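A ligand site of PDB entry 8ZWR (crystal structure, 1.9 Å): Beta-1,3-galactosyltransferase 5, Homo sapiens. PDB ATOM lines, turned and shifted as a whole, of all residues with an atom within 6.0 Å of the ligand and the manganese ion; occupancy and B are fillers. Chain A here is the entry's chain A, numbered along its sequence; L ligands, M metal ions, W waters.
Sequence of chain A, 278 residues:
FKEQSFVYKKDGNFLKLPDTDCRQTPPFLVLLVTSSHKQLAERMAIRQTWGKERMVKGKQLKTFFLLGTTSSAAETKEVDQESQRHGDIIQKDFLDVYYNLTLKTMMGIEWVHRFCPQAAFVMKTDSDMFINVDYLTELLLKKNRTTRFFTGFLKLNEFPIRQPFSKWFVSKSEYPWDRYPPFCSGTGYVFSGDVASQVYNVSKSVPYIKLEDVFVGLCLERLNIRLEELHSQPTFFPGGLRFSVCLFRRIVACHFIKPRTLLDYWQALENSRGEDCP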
ATOM      1  N   THR A  34      10.157 -28.214 -14.434  1.00  0.00           N
ATOM      2  CA  THR A  34      11.615 -28.182 -14.587  1.00  0.00           C
ATOM      3  C   THR A  34      12.276 -28.966 -13.462  1.00  0.00           C
ATOM      4  O   THR A  34      11.825 -28.939 -12.299  1.00  0.00           O
ATOM      5  CB  THR A  34      12.160 -26.752 -14.624  1.00  0.00           C
ATOM      6  OG1 THR A  34      11.925 -26.078 -13.376  1.00  0.00           O
ATOM      7  CG2 THR A  34      11.507 -25.953 -15.752  1.00  0.00           C
ATOM      8  N   SER A  35      13.317 -29.706 -13.825  1.00  0.00           N
ATOM      9  CA  SER A  35      14.194 -30.417 -12.914  1.00  0.00           C
ATOM     10  C   SER A  35      15.459 -30.738 -13.696  1.00  0.00           C
ATOM     11  O   SER A  35      15.422 -30.831 -14.924  1.00  0.00           O
ATOM     12  CB  SER A  35      13.561 -31.707 -12.360  1.00  0.00           C
ATOM     13  OG  SER A  35      13.272 -32.655 -13.382  1.00  0.00           O
ATOM     14  N   SER A  36      16.582 -30.872 -13.001  1.00  0.00           N
ATOM     15  CA  SER A  36      17.812 -31.299 -13.646  1.00  0.00           C
ATOM     16  C   SER A  36      17.859 -32.825 -13.771  1.00  0.00           C
ATOM     17  O   SER A  36      17.089 -33.542 -13.141  1.00  0.00           O
ATOM     18  CB  SER A  36      19.013 -30.788 -12.870  1.00  0.00           C
ATOM     19  OG  SER A  36      19.165 -31.551 -11.699  1.00  0.00           O
ATOM     20  N   HIS A  37      18.800 -33.330 -14.570  1.00  0.00           N
ATOM     21  CA  HIS A  37      18.870 -34.776 -14.800  1.00  0.00           C
ATOM     22  C   HIS A  37      18.968 -35.588 -13.517  1.00  0.00           C
ATOM     23  O   HIS A  37      18.310 -36.625 -13.378  1.00  0.00           O
ATOM     24  CB  HIS A  37      20.075 -35.126 -15.682  1.00  0.00           C
ATOM     25  CG  HIS A  37      19.883 -34.774 -17.113  1.00  0.00           C
ATOM     26  ND1 HIS A  37      19.608 -35.716 -18.076  1.00  0.00           N
ATOM     27  CD2 HIS A  37      19.885 -33.575 -17.737  1.00  0.00           C
ATOM     28  CE1 HIS A  37      19.473 -35.115 -19.246  1.00  0.00           C
ATOM     29  NE2 HIS A  37      19.635 -33.816 -19.068  1.00  0.00           N
ATOM     30  N   GLN A  39      17.829 -35.105 -10.656  1.00  0.00           N
ATOM     31  CA  GLN A  39      16.724 -34.947  -9.704  1.00  0.00           C
ATOM     32  C   GLN A  39      15.607 -35.954  -9.959  1.00  0.00           C
ATOM     33  O   GLN A  39      14.437 -35.580 -10.064  1.00  0.00           O
ATOM     34  CB  GLN A  39      16.223 -33.502  -9.755  1.00  0.00           C
ATOM     35  CG  GLN A  39      17.228 -32.520  -9.168  1.00  0.00           C
ATOM     36  CD  GLN A  39      16.752 -31.076  -9.192  1.00  0.00           C
ATOM     37  OE1 GLN A  39      16.480 -30.514 -10.262  1.00  0.00           O
ATOM     38  NE2 GLN A  39      16.622 -30.485  -8.015  1.00  0.00           N
ATOM     39  N   LEU A  66      10.389 -31.222 -18.314  1.00  0.00           N
ATOM     40  CA  LEU A  66      11.286 -30.587 -19.275  1.00  0.00           C
ATOM     41  C   LEU A  66      12.729 -30.964 -18.932  1.00  0.00           C
ATOM     42  O   LEU A  66      13.159 -30.809 -17.780  1.00  0.00           O
ATOM     43  CB  LEU A  66      11.116 -29.073 -19.234  1.00  0.00           C
ATOM     44  CG  LEU A  66       9.673 -28.581 -19.340  1.00  0.00           C
ATOM     45  CD1 LEU A  66       9.576 -27.049 -19.311  1.00  0.00           C
ATOM     46  CD2 LEU A  66       9.005 -29.124 -20.603  1.00  0.00           C
ATOM     47  N   ASP A  96      21.789 -28.888 -20.011  1.00  0.00           N
ATOM     48  CA  ASP A  96      20.824 -28.659 -18.936  1.00  0.00           C
ATOM     49  C   ASP A  96      21.562 -28.164 -17.691  1.00  0.00           C
ATOM     50  O   ASP A  96      21.998 -28.954 -16.854  1.00  0.00           O
ATOM     51  CB  ASP A  96      20.037 -29.929 -18.678  1.00  0.00           C
ATOM     52  CG  ASP A  96      18.720 -29.672 -17.923  1.00  0.00           C
ATOM     53  OD1 ASP A  96      18.613 -28.658 -17.212  1.00  0.00           O
ATOM     54  OD2 ASP A  96      17.793 -30.502 -18.022  1.00  0.00           O
ATOM     55  N   VAL A  97      21.696 -26.838 -17.552  1.00  0.00           N
ATOM     56  CA  VAL A  97      22.327 -26.174 -16.410  1.00  0.00           C
ATOM     57  C   VAL A  97      21.462 -24.978 -15.996  1.00  0.00           C
ATOM     58  O   VAL A  97      20.598 -24.525 -16.738  1.00  0.00           O
ATOM     59  CB  VAL A  97      23.775 -25.701 -16.740  1.00  0.00           C
ATOM     60  CG1 VAL A  97      24.708 -26.875 -16.966  1.00  0.00           C
ATOM     61  CG2 VAL A  97      23.778 -24.782 -17.947  1.00  0.00           C
ATOM     62  N   TYR A  98      21.644 -24.531 -14.744  1.00  0.00           N
ATOM     63  CA  TYR A  98      20.845 -23.429 -14.225  1.00  0.00           C
ATOM     64  C   TYR A  98      20.764 -22.252 -15.205  1.00  0.00           C
ATOM     65  O   TYR A  98      19.665 -21.733 -15.489  1.00  0.00           O
ATOM     66  CB  TYR A  98      21.382 -22.942 -12.867  1.00  0.00           C
ATOM     67  CG  TYR A  98      20.475 -21.931 -12.231  1.00  0.00           C
ATOM     68  CD1 TYR A  98      19.274 -22.309 -11.648  1.00  0.00           C
ATOM     69  CD2 TYR A  98      20.809 -20.595 -12.237  1.00  0.00           C
ATOM     70  CE1 TYR A  98      18.407 -21.381 -11.084  1.00  0.00           C
ATOM     71  CE2 TYR A  98      19.959 -19.653 -11.664  1.00  0.00           C
ATOM     72  CZ  TYR A  98      18.758 -20.061 -11.094  1.00  0.00           C
ATOM     73  OH  TYR A  98      17.951 -19.095 -10.546  1.00  0.00           O
ATOM     74  N   LEU A 101      18.197 -22.254 -18.097  1.00  0.00           N
ATOM     75  CA  LEU A 101      16.765 -22.392 -17.874  1.00  0.00           C
ATOM     76  C   LEU A 101      15.928 -21.643 -18.915  1.00  0.00           C
ATOM     77  O   LEU A 101      14.802 -22.081 -19.204  1.00  0.00           O
ATOM     78  CB  LEU A 101      16.412 -21.903 -16.473  1.00  0.00           C
ATOM     79  CG  LEU A 101      16.766 -22.981 -15.444  1.00  0.00           C
ATOM     80  CD1 LEU A 101      16.510 -22.479 -14.019  1.00  0.00           C
ATOM     81  CD2 LEU A 101      16.009 -24.287 -15.736  1.00  0.00           C
ATOM     82  N   THR A 102      16.422 -20.549 -19.491  1.00  0.00           N
ATOM     83  CA  THR A 102      15.614 -19.865 -20.510  1.00  0.00           C
ATOM     84  C   THR A 102      15.325 -20.786 -21.698  1.00  0.00           C
ATOM     85  O   THR A 102      14.164 -20.891 -22.138  1.00  0.00           O
ATOM     86  CB  THR A 102      16.288 -18.554 -20.927  1.00  0.00           C
ATOM     87  OG1 THR A 102      16.365 -17.681 -19.777  1.00  0.00           O
ATOM     88  CG2 THR A 102      15.504 -17.861 -22.070  1.00  0.00           C
ATOM     89  N   LYS A 104      15.255 -24.040 -21.545  1.00  0.00           N
ATOM     90  CA  LYS A 104      14.324 -25.056 -21.073  1.00  0.00           C
ATOM     91  C   LYS A 104      12.901 -24.531 -21.128  1.00  0.00           C
ATOM     92  O   LYS A 104      11.998 -25.193 -21.670  1.00  0.00           O
ATOM     93  CB  LYS A 104      14.686 -25.509 -19.665  1.00  0.00           C
ATOM     94  CG  LYS A 104      13.782 -26.640 -19.192  1.00  0.00           C
ATOM     95  CD  LYS A 104      14.271 -27.277 -17.927  1.00  0.00           C
ATOM     96  CE  LYS A 104      15.542 -28.094 -18.135  1.00  0.00           C
ATOM     97  NZ  LYS A 104      15.656 -29.158 -17.067  1.00  0.00           N
ATOM     98  N   LYS A 124       3.881 -23.434 -16.026  1.00  0.00           N
ATOM     99  CA  LYS A 124       5.303 -23.726 -15.938  1.00  0.00           C
ATOM    100  C   LYS A 124       5.695 -23.711 -14.467  1.00  0.00           C
ATOM    101  O   LYS A 124       5.414 -22.737 -13.751  1.00  0.00           O
ATOM    102  CB  LYS A 124       6.141 -22.722 -16.742  1.00  0.00           C
ATOM    103  CG  LYS A 124       7.670 -22.936 -16.644  1.00  0.00           C
ATOM    104  CD  LYS A 124       8.280 -22.243 -15.416  1.00  0.00           C
ATOM    105  CE  LYS A 124       9.722 -22.678 -15.131  1.00  0.00           C
ATOM    106  NZ  LYS A 124      10.323 -21.937 -13.983  1.00  0.00           N
ATOM    107  N   THR A 125       6.308 -24.802 -13.990  1.00  0.00           N
ATOM    108  CA  THR A 125       6.656 -24.849 -12.575  1.00  0.00           C
ATOM    109  C   THR A 125       7.959 -25.609 -12.356  1.00  0.00           C
ATOM    110  O   THR A 125       8.527 -26.182 -13.289  1.00  0.00           O
ATOM    111  CB  THR A 125       5.496 -25.408 -11.764  1.00  0.00           C
ATOM    112  OG1 THR A 125       5.734 -25.132 -10.387  1.00  0.00           O
ATOM    113  CG2 THR A 125       5.301 -26.929 -11.976  1.00  0.00           C
ATOM    114  N   ASP A 126       8.436 -25.581 -11.117  1.00  0.00           N
ATOM    115  CA  ASP A 126       9.721 -26.121 -10.720  1.00  0.00           C
ATOM    116  C   ASP A 126       9.563 -27.349  -9.828  1.00  0.00           C
ATOM    117  O   ASP A 126       8.460 -27.737  -9.463  1.00  0.00           O
ATOM    118  CB  ASP A 126      10.540 -25.047 -10.007  1.00  0.00           C
ATOM    119  CG  ASP A 126      10.923 -23.908 -10.938  1.00  0.00           C
ATOM    120  OD1 ASP A 126      10.837 -24.074 -12.195  1.00  0.00           O
ATOM    121  OD2 ASP A 126      11.335 -22.857 -10.422  1.00  0.00           O
ATOM    122  N   SER A 127      10.679 -28.000  -9.532  1.00  0.00           N
ATOM    123  CA  SER A 127      10.640 -29.300  -8.881  1.00  0.00           C
ATOM    124  C   SER A 127      10.666 -29.206  -7.357  1.00  0.00           C
ATOM    125  O   SER A 127      10.502 -30.231  -6.689  1.00  0.00           O
ATOM    126  CB  SER A 127      11.817 -30.151  -9.364  1.00  0.00           C
ATOM    127  OG  SER A 127      13.041 -29.444  -9.195  1.00  0.00           O
ATOM    128  N   ASP A 128      10.880 -28.003  -6.802  1.00  0.00           N
ATOM    129  CA  ASP A 128      10.922 -27.783  -5.365  1.00  0.00           C
ATOM    130  C   ASP A 128       9.617 -27.156  -4.879  1.00  0.00           C
ATOM    131  O   ASP A 128       9.607 -26.225  -4.064  1.00  0.00           O
ATOM    132  CB  ASP A 128      12.132 -26.912  -4.985  1.00  0.00           C
ATOM    133  CG  ASP A 128      12.272 -25.660  -5.869  1.00  0.00           C
ATOM    134  OD1 ASP A 128      11.459 -25.472  -6.792  1.00  0.00           O
ATOM    135  OD2 ASP A 128      13.225 -24.849  -5.663  1.00  0.00           O
ATOM    136  N   LYS A 167      23.442 -15.723  -6.988  1.00  0.00           N
ATOM    137  CA  LYS A 167      22.891 -16.684  -7.944  1.00  0.00           C
ATOM    138  C   LYS A 167      22.096 -15.985  -9.053  1.00  0.00           C
ATOM    139  O   LYS A 167      22.074 -16.474 -10.194  1.00  0.00           O
ATOM    140  CB  LYS A 167      22.023 -17.682  -7.187  1.00  0.00           C
ATOM    141  CG  LYS A 167      21.278 -18.695  -8.059  1.00  0.00           C
ATOM    142  CD  LYS A 167      20.555 -19.703  -7.169  1.00  0.00           C
ATOM    143  CE  LYS A 167      20.047 -20.911  -7.958  1.00  0.00           C
ATOM    144  NZ  LYS A 167      19.457 -21.966  -7.085  1.00  0.00           N
ATOM    145  N   TRP A 168      21.463 -14.874  -8.742  1.00  0.00           N
ATOM    146  CA  TRP A 168      20.668 -14.151  -9.764  1.00  0.00           C
ATOM    147  C   TRP A 168      21.329 -12.849 -10.386  1.00  0.00           C
ATOM    148  O   TRP A 168      20.691 -11.944 -10.991  1.00  0.00           O
ATOM    149  CB  TRP A 168      19.284 -13.842  -9.187  1.00  0.00           C
ATOM    150  CG  TRP A 168      18.695 -15.071  -8.543  1.00  0.00           C
ATOM    151  CD1 TRP A 168      18.006 -16.093  -9.154  1.00  0.00           C
ATOM    152  CD2 TRP A 168      18.823 -15.447  -7.167  1.00  0.00           C
ATOM    153  NE1 TRP A 168      17.660 -17.057  -8.240  1.00  0.00           N
ATOM    154  CE2 TRP A 168      18.153 -16.686  -7.006  1.00  0.00           C
ATOM    155  CE3 TRP A 168      19.425 -14.852  -6.049  1.00  0.00           C
ATOM    156  CZ2 TRP A 168      18.080 -17.349  -5.769  1.00  0.00           C
ATOM    157  CZ3 TRP A 168      19.342 -15.518  -4.815  1.00  0.00           C
ATOM    158  CH2 TRP A 168      18.679 -16.741  -4.690  1.00  0.00           C
ATOM    159  N   SER A 185       7.083 -14.858 -10.742  1.00  0.00           N
ATOM    160  CA  SER A 185       8.108 -15.813 -10.250  1.00  0.00           C
ATOM    161  C   SER A 185       8.097 -17.093 -11.109  1.00  0.00           C
ATOM    162  O   SER A 185       7.036 -17.658 -11.296  1.00  0.00           O
ATOM    163  CB  SER A 185       7.999 -16.145  -8.757  1.00  0.00           C
ATOM    164  OG  SER A 185       8.737 -17.307  -8.430  1.00  0.00           O
ATOM    165  N   GLY A 186       9.263 -17.534 -11.562  1.00  0.00           N
ATOM    166  CA  GLY A 186       9.375 -18.819 -12.289  1.00  0.00           C
ATOM    167  C   GLY A 186       9.010 -20.024 -11.438  1.00  0.00           C
ATOM    168  O   GLY A 186       8.837 -21.107 -11.978  1.00  0.00           O
ATOM    169  N   THR A 187       8.938 -19.843 -10.127  1.00  0.00           N
ATOM    170  CA  THR A 187       8.555 -20.949  -9.226  1.00  0.00           C
ATOM    171  C   THR A 187       7.277 -21.626  -9.712  1.00  0.00           C
ATOM    172  O   THR A 187       7.177 -22.836  -9.553  1.00  0.00           O
ATOM    173  CB  THR A 187       8.389 -20.444  -7.784  1.00  0.00           C
ATOM    174  OG1 THR A 187       7.430 -19.398  -7.694  1.00  0.00           O
ATOM    175  CG2 THR A 187       9.727 -19.976  -7.221  1.00  0.00           C
ATOM    176  N   GLY A 188       6.335 -20.842 -10.240  1.00  0.00           N
ATOM    177  CA  GLY A 188       5.090 -21.392 -10.798  1.00  0.00           C
ATOM    178  C   GLY A 188       4.238 -20.289 -11.381  1.00  0.00           C
ATOM    179  O   GLY A 188       3.746 -19.472 -10.617  1.00  0.00           O
ATOM    180  N   LYS A 210      19.268 -14.691 -19.133  1.00  0.00           N
ATOM    181  CA  LYS A 210      19.433 -16.053 -18.580  1.00  0.00           C
ATOM    182  C   LYS A 210      18.388 -16.404 -17.493  1.00  0.00           C
ATOM    183  O   LYS A 210      18.316 -17.563 -17.140  1.00  0.00           O
ATOM    184  CB  LYS A 210      20.835 -16.140 -17.967  1.00  0.00           C
ATOM    185  CG  LYS A 210      21.194 -15.220 -16.833  1.00  0.00           C
ATOM    186  CD  LYS A 210      22.689 -15.333 -16.554  1.00  0.00           C
ATOM    187  CE  LYS A 210      23.094 -14.573 -15.336  1.00  0.00           C
ATOM    188  NZ  LYS A 210      24.536 -14.302 -15.302  1.00  0.00           N
ATOM    189  N   LEU A 211      17.698 -15.416 -16.958  1.00  0.00           N
ATOM    190  CA  LEU A 211      16.587 -15.686 -16.002  1.00  0.00           C
ATOM    191  C   LEU A 211      15.295 -15.917 -16.808  1.00  0.00           C
ATOM    192  O   LEU A 211      14.810 -14.951 -17.403  1.00  0.00           O
ATOM    193  CB  LEU A 211      16.495 -14.548 -15.004  1.00  0.00           C
ATOM    194  CG  LEU A 211      17.809 -14.180 -14.311  1.00  0.00           C
ATOM    195  CD1 LEU A 211      17.678 -12.924 -13.457  1.00  0.00           C
ATOM    196  CD2 LEU A 211      18.363 -15.331 -13.507  1.00  0.00           C
ATOM    197  N   GLU A 212      14.791 -17.147 -16.822  1.00  0.00           N
ATOM    198  CA  GLU A 212      13.628 -17.537 -17.683  1.00  0.00           C
ATOM    199  C   GLU A 212      12.366 -16.709 -17.401  1.00  0.00           C
ATOM    200  O   GLU A 212      11.731 -16.277 -18.363  1.00  0.00           O
ATOM    201  CB  GLU A 212      13.416 -19.045 -17.517  1.00  0.00           C
ATOM    202  CG  GLU A 212      12.919 -19.476 -16.151  1.00  0.00           C
ATOM    203  CD  GLU A 212      11.401 -19.420 -16.082  1.00  0.00           C
ATOM    204  OE1 GLU A 212      10.777 -19.331 -17.133  1.00  0.00           O
ATOM    205  OE2 GLU A 212      10.859 -19.436 -14.977  1.00  0.00           O
ATOM    206  N   ASP A 213      12.015 -16.520 -16.129  1.00  0.00           N
ATOM    207  CA  ASP A 213      10.809 -15.729 -15.753  1.00  0.00           C
ATOM    208  C   ASP A 213      10.923 -14.286 -16.263  1.00  0.00           C
ATOM    209  O   ASP A 213       9.944 -13.766 -16.777  1.00  0.00           O
ATOM    210  CB  ASP A 213      10.525 -15.805 -14.272  1.00  0.00           C
ATOM    211  CG  ASP A 213      11.690 -15.582 -13.317  1.00  0.00           C
ATOM    212  OD1 ASP A 213      12.802 -15.274 -13.792  1.00  0.00           O
ATOM    213  OD2 ASP A 213      11.482 -15.705 -12.095  1.00  0.00           O
ATOM    214  N   VAL A 214      12.094 -13.677 -16.124  1.00  0.00           N
ATOM    215  CA  VAL A 214      12.284 -12.300 -16.659  1.00  0.00           C
ATOM    216  C   VAL A 214      12.099 -12.345 -18.192  1.00  0.00           C
ATOM    217  O   VAL A 214      11.386 -11.495 -18.714  1.00  0.00           O
ATOM    218  CB  VAL A 214      13.610 -11.637 -16.213  1.00  0.00           C
ATOM    219  CG1 VAL A 214      13.763 -10.235 -16.789  1.00  0.00           C
ATOM    220  CG2 VAL A 214      13.741 -11.614 -14.700  1.00  0.00           C
ATOM    221  N   HIS A 255       6.773 -22.695  -2.616  1.00  0.00           N
ATOM    222  CA  HIS A 255       8.166 -22.961  -2.963  1.00  0.00           C
ATOM    223  C   HIS A 255       8.911 -23.480  -1.720  1.00  0.00           C
ATOM    224  O   HIS A 255       8.333 -23.593  -0.630  1.00  0.00           O
ATOM    225  CB  HIS A 255       8.760 -21.679  -3.562  1.00  0.00           C
ATOM    226  CG  HIS A 255      10.188 -21.769  -4.026  1.00  0.00           C
ATOM    227  ND1 HIS A 255      11.131 -20.839  -3.660  1.00  0.00           N
ATOM    228  CD2 HIS A 255      10.792 -22.592  -4.915  1.00  0.00           C
ATOM    229  CE1 HIS A 255      12.287 -21.110  -4.253  1.00  0.00           C
ATOM    230  NE2 HIS A 255      12.105 -22.177  -5.030  1.00  0.00           N
ATOM    231  N   PHE A 256      10.168 -23.878  -1.896  1.00  0.00           N
ATOM    232  CA  PHE A 256      11.030 -24.378  -0.810  1.00  0.00           C
ATOM    233  C   PHE A 256      10.552 -25.709  -0.243  1.00  0.00           C
ATOM    234  O   PHE A 256      10.578 -25.905   0.969  1.00  0.00           O
ATOM    235  CB  PHE A 256      11.163 -23.341   0.343  1.00  0.00           C
ATOM    236  CG  PHE A 256      11.930 -22.083  -0.057  1.00  0.00           C
ATOM    237  CD1 PHE A 256      13.200 -22.173  -0.639  1.00  0.00           C
ATOM    238  CD2 PHE A 256      11.350 -20.815   0.089  1.00  0.00           C
ATOM    239  CE1 PHE A 256      13.887 -21.020  -1.010  1.00  0.00           C
ATOM    240  CE2 PHE A 256      12.046 -19.659  -0.312  1.00  0.00           C
ATOM    241  CZ  PHE A 256      13.308 -19.781  -0.844  1.00  0.00           C
HETATM  242  N1  LIG L   1      16.754 -26.887 -12.821  1.00  0.00           N
HETATM  243  C1  LIG L   1      16.865 -27.470 -13.976  1.00  0.00           C
HETATM  244  N2  LIG L   1      18.084 -27.687 -14.535  1.00  0.00           N
HETATM  245  C2  LIG L   1      19.186 -27.316 -13.926  1.00  0.00           C
HETATM  246  C3  LIG L   1      19.107 -26.666 -12.680  1.00  0.00           C
HETATM  247  C4  LIG L   1      17.854 -26.450 -12.151  1.00  0.00           C
HETATM  248  O1  LIG L   1      15.952 -27.808 -14.525  1.00  0.00           O
HETATM  249  O2  LIG L   1      20.189 -27.506 -14.391  1.00  0.00           O
HETATM  250  C5  LIG L   1      15.415 -26.629 -12.213  1.00  0.00           C
HETATM  251  C6  LIG L   1      15.428 -26.902 -10.893  1.00  0.00           C
HETATM  252  O3  LIG L   1      15.177 -28.269 -10.597  1.00  0.00           O
HETATM  253  C7  LIG L   1      14.268 -26.038 -10.367  1.00  0.00           C
HETATM  254  C8  LIG L   1      14.374 -24.746 -11.241  1.00  0.00           C
HETATM  255  O4  LIG L   1      15.096 -25.054 -12.296  1.00  0.00           O
HETATM  256  O5  LIG L   1      13.114 -26.638 -10.609  1.00  0.00           O
HETATM  257  C9  LIG L   1      14.949 -23.572 -10.509  1.00  0.00           C
HETATM  258  O6  LIG L   1      16.197 -23.898  -9.939  1.00  0.00           O
HETATM  259  P1  LIG L   1      16.476 -23.473  -8.347  1.00  0.00           P
HETATM  260  O7  LIG L   1      17.795 -24.134  -7.894  1.00  0.00           O
HETATM  261  O8  LIG L   1      15.283 -23.968  -7.437  1.00  0.00           O
HETATM  262  O9  LIG L   1      16.706 -21.821  -8.215  1.00  0.00           O
HETATM  263  P2  LIG L   1      15.580 -20.665  -8.155  1.00  0.00           P
HETATM  264  O10 LIG L   1      14.471 -20.985  -7.276  1.00  0.00           O
HETATM  265  O11 LIG L   1      16.257 -19.402  -7.697  1.00  0.00           O
HETATM  266  O12 LIG L   1      15.140 -20.378  -9.671  1.00  0.00           O
HETATM  267  C10 LIG L   1      14.406 -19.155  -9.950  1.00  0.00           C
HETATM  268  C11 LIG L   1      12.997 -19.556 -10.398  1.00  0.00           C
HETATM  269  C12 LIG L   1      13.081 -20.349 -11.615  1.00  0.00           C
HETATM  270  C13 LIG L   1      13.758 -19.635 -12.694  1.00  0.00           C
HETATM  271  C14 LIG L   1      15.141 -19.134 -12.241  1.00  0.00           C
HETATM  272  C15 LIG L   1      15.750 -18.160 -13.332  1.00  0.00           C
HETATM  273  F1  LIG L   1      12.419 -20.214  -9.375  1.00  0.00           F
HETATM  274  O13 LIG L   1      11.836 -20.833 -12.045  1.00  0.00           O
HETATM  275  O14 LIG L   1      12.989 -18.537 -13.154  1.00  0.00           O
HETATM  276  O15 LIG L   1      15.102 -18.425 -10.996  1.00  0.00           O
HETATM  277  O16 LIG L   1      15.860 -18.842 -14.585  1.00  0.00           O
HETATM  278 MN    MN M   1      13.742 -22.871  -6.343  1.00  0.00          MN
HETATM  279  O   HOH W   1      15.352 -22.449  -4.435  1.00  0.00           O
HETATM  280  O   HOH W   2      15.510 -26.544  -6.618  1.00  0.00           O
HETATM  281  O   HOH W   3      12.724 -22.839 -14.335  1.00  0.00           O
HETATM  282  O   HOH W   4      19.494 -25.421  -9.669  1.00  0.00           O
HETATM  283  O   HOH W   5      22.367 -28.762 -12.839  1.00  0.00           O
HETATM  284  O   HOH W   6      12.941 -18.546  -6.698  1.00  0.00           O
HETATM  285  O   HOH W   7      11.919 -23.158  -7.957  1.00  0.00           O
HETATM  286  O   HOH W   8      18.030 -27.379  -8.464  1.00  0.00           O
HETATM  287  O   HOH W   9      18.582 -19.118 -14.940  1.00  0.00           O
HETATM  288  O   HOH W  10      16.692 -20.098  -5.241  1.00  0.00           O
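Water W7 lies within hydrogen-bond range of OD2 of Asp 126 (2.6 Å) and OD1 of Asp 128 (2.6 Å).
Water W9 lies within hydrogen-bond range of O of Lys 210 (2.7 Å), O16 of the ligand (2.8 Å) and O of Tyr 98 (2.9 Å).
Water W3 lies within hydrogen-bond range of NZ of Lys 124, OD1 of Asp 126, O13 of the ligand and OG1 of Thr 34.
Water W8 lies within hydrogen-bond range of an oxygen (O7) of the ligand (3.3 Å) and the side-chain amide nitrogen of Gln 39 (3.4 Å).
Val 97 touches the ligand.
Leu 101 touches the ligand.
Thr 187 touches the ligand (CG2 to F1, 3.5 Å).
O of Lys 210 touches O16 of the ligand (3.8 Å).
CA of Leu 211 touches O16 of the ligand, at 3.5 Å.
Hydrophobic or aromatic side chains that line the ligand: Tyr 98, Leu 101, Trp 168, Leu 211 and His 255.
OD2 of Asp 128 binds the manganese ion.
The manganese ion is bound by O8 of the ligand (2.2 Å).
A ring nitrogen (NE2) of His 255 binds the manganese ion, at 2.2 Å.
An oxygen (O10) of the ligand is bound to the manganese ion (2.2 Å).
Water W7 binds the manganese ion.
Water W1 binds the manganese ion (2.5 Å).
The manganese ion has six donor atoms within binding distance.
Of the 30 residues printed, 2 come within 4 Å of the manganese ion.
The backbone carbonyl oxygen of Asp 128 is in hydrogen-bond range of the backbone NH of Phe 256, 3.2 Å away.
N of Gly 186 lies within hydrogen-bond range of OD2 of Asp 213 (2.9 Å).
The side-chain amino group (NZ) of Lys 104 is in salt-bridge range of the side-chain carboxylate (OD2) of Asp 96 (2.7 Å).
N of Ser 127 sits at hydrogen-bond distance from O of Thr 34 (3.1 Å).
OG1 of Thr 187 lies within hydrogen-bond range of OG of Ser 185, 2.6 Å away.
OD1 of Asp 126 lies within hydrogen-bond range of OG1 of Thr 34 (2.6 Å).
The side-chain carboxylate of Asp 126 is in salt-bridge range of the side-chain amino group of Lys 124, at 2.8 Å.
The backbone carbonyl oxygen of Thr 187 is in hydrogen-bond range of the backbone NH of Asp 126, 3.4 Å away.
An oxygen (O13) of the ligand sits close to the backbone carbonyl oxygen (O) of Gly 186 (3.0 Å).
The backbone NH (N) of Tyr 98 lies within hydrogen-bond range of an oxygen (O2) of the ligand, at 3.3 Å.
An oxygen (O7) of the ligand lies within salt-bridge range of the side-chain amino group of Lys 167 (2.8 Å).
The side-chain hydroxyl (OH) of Tyr 98 lies within hydrogen-bond range of an oxygen (O15) of the ligand.
OD2 of Asp 126 sits at hydrogen-bond distance from O13 of the ligand, 2.6 Å away.
O14 of the ligand sits close to OD1 of Asp 213 (3.3 Å).
The backbone NH (N) of Glu 212 is in hydrogen-bond range of an oxygen (O16) of the ligand (3.0 Å).
N of Ser 36 is in hydrogen-bond range of O1 of the ligand (3.5 Å).
An oxygen (O1) of the ligand lies close to the backbone NH (N) of Ser 35 (3.3 Å).
NE1 of Trp 168 sits at hydrogen-bond distance from O11 of the ligand, at 2.8 Å.
The side-chain hydroxyl (OG) of Ser 127 is in hydrogen-bond range of an oxygen (O3) of the ligand, 2.8 Å away.
An oxygen (O5) of the ligand lies within hydrogen-bond range of the side-chain hydroxyl (OG1) of Thr 34, 3.1 Å away.
The side-chain carboxylate of Asp 96 is in hydrogen-bond range of a nitrogen (N2) of the ligand, at 2.9 Å.
O of Thr 34 sits at hydrogen-bond distance from O5 of the ligand (3.1 Å).
The side-chain amide oxygen (OE1) of Gln 39 lies within hydrogen-bond range of an oxygen (O3) of the ligand.
The side-chain carboxylate (OE2) of Glu 212 sits at hydrogen-bond distance from an oxygen (O14) of the ligand, at 2.9 Å.
NZ of Lys 124 lies within hydrogen-bond range of O13 of the ligand (2.7 Å).
The side-chain amino group (NZ) of Lys 104 sits at hydrogen-bond distance from an oxygen (O1) of the ligand (2.9 Å).
The backbone NH (N) of Ser 127 is in hydrogen-bond range of an oxygen (O5) of the ligand (3.0 Å).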
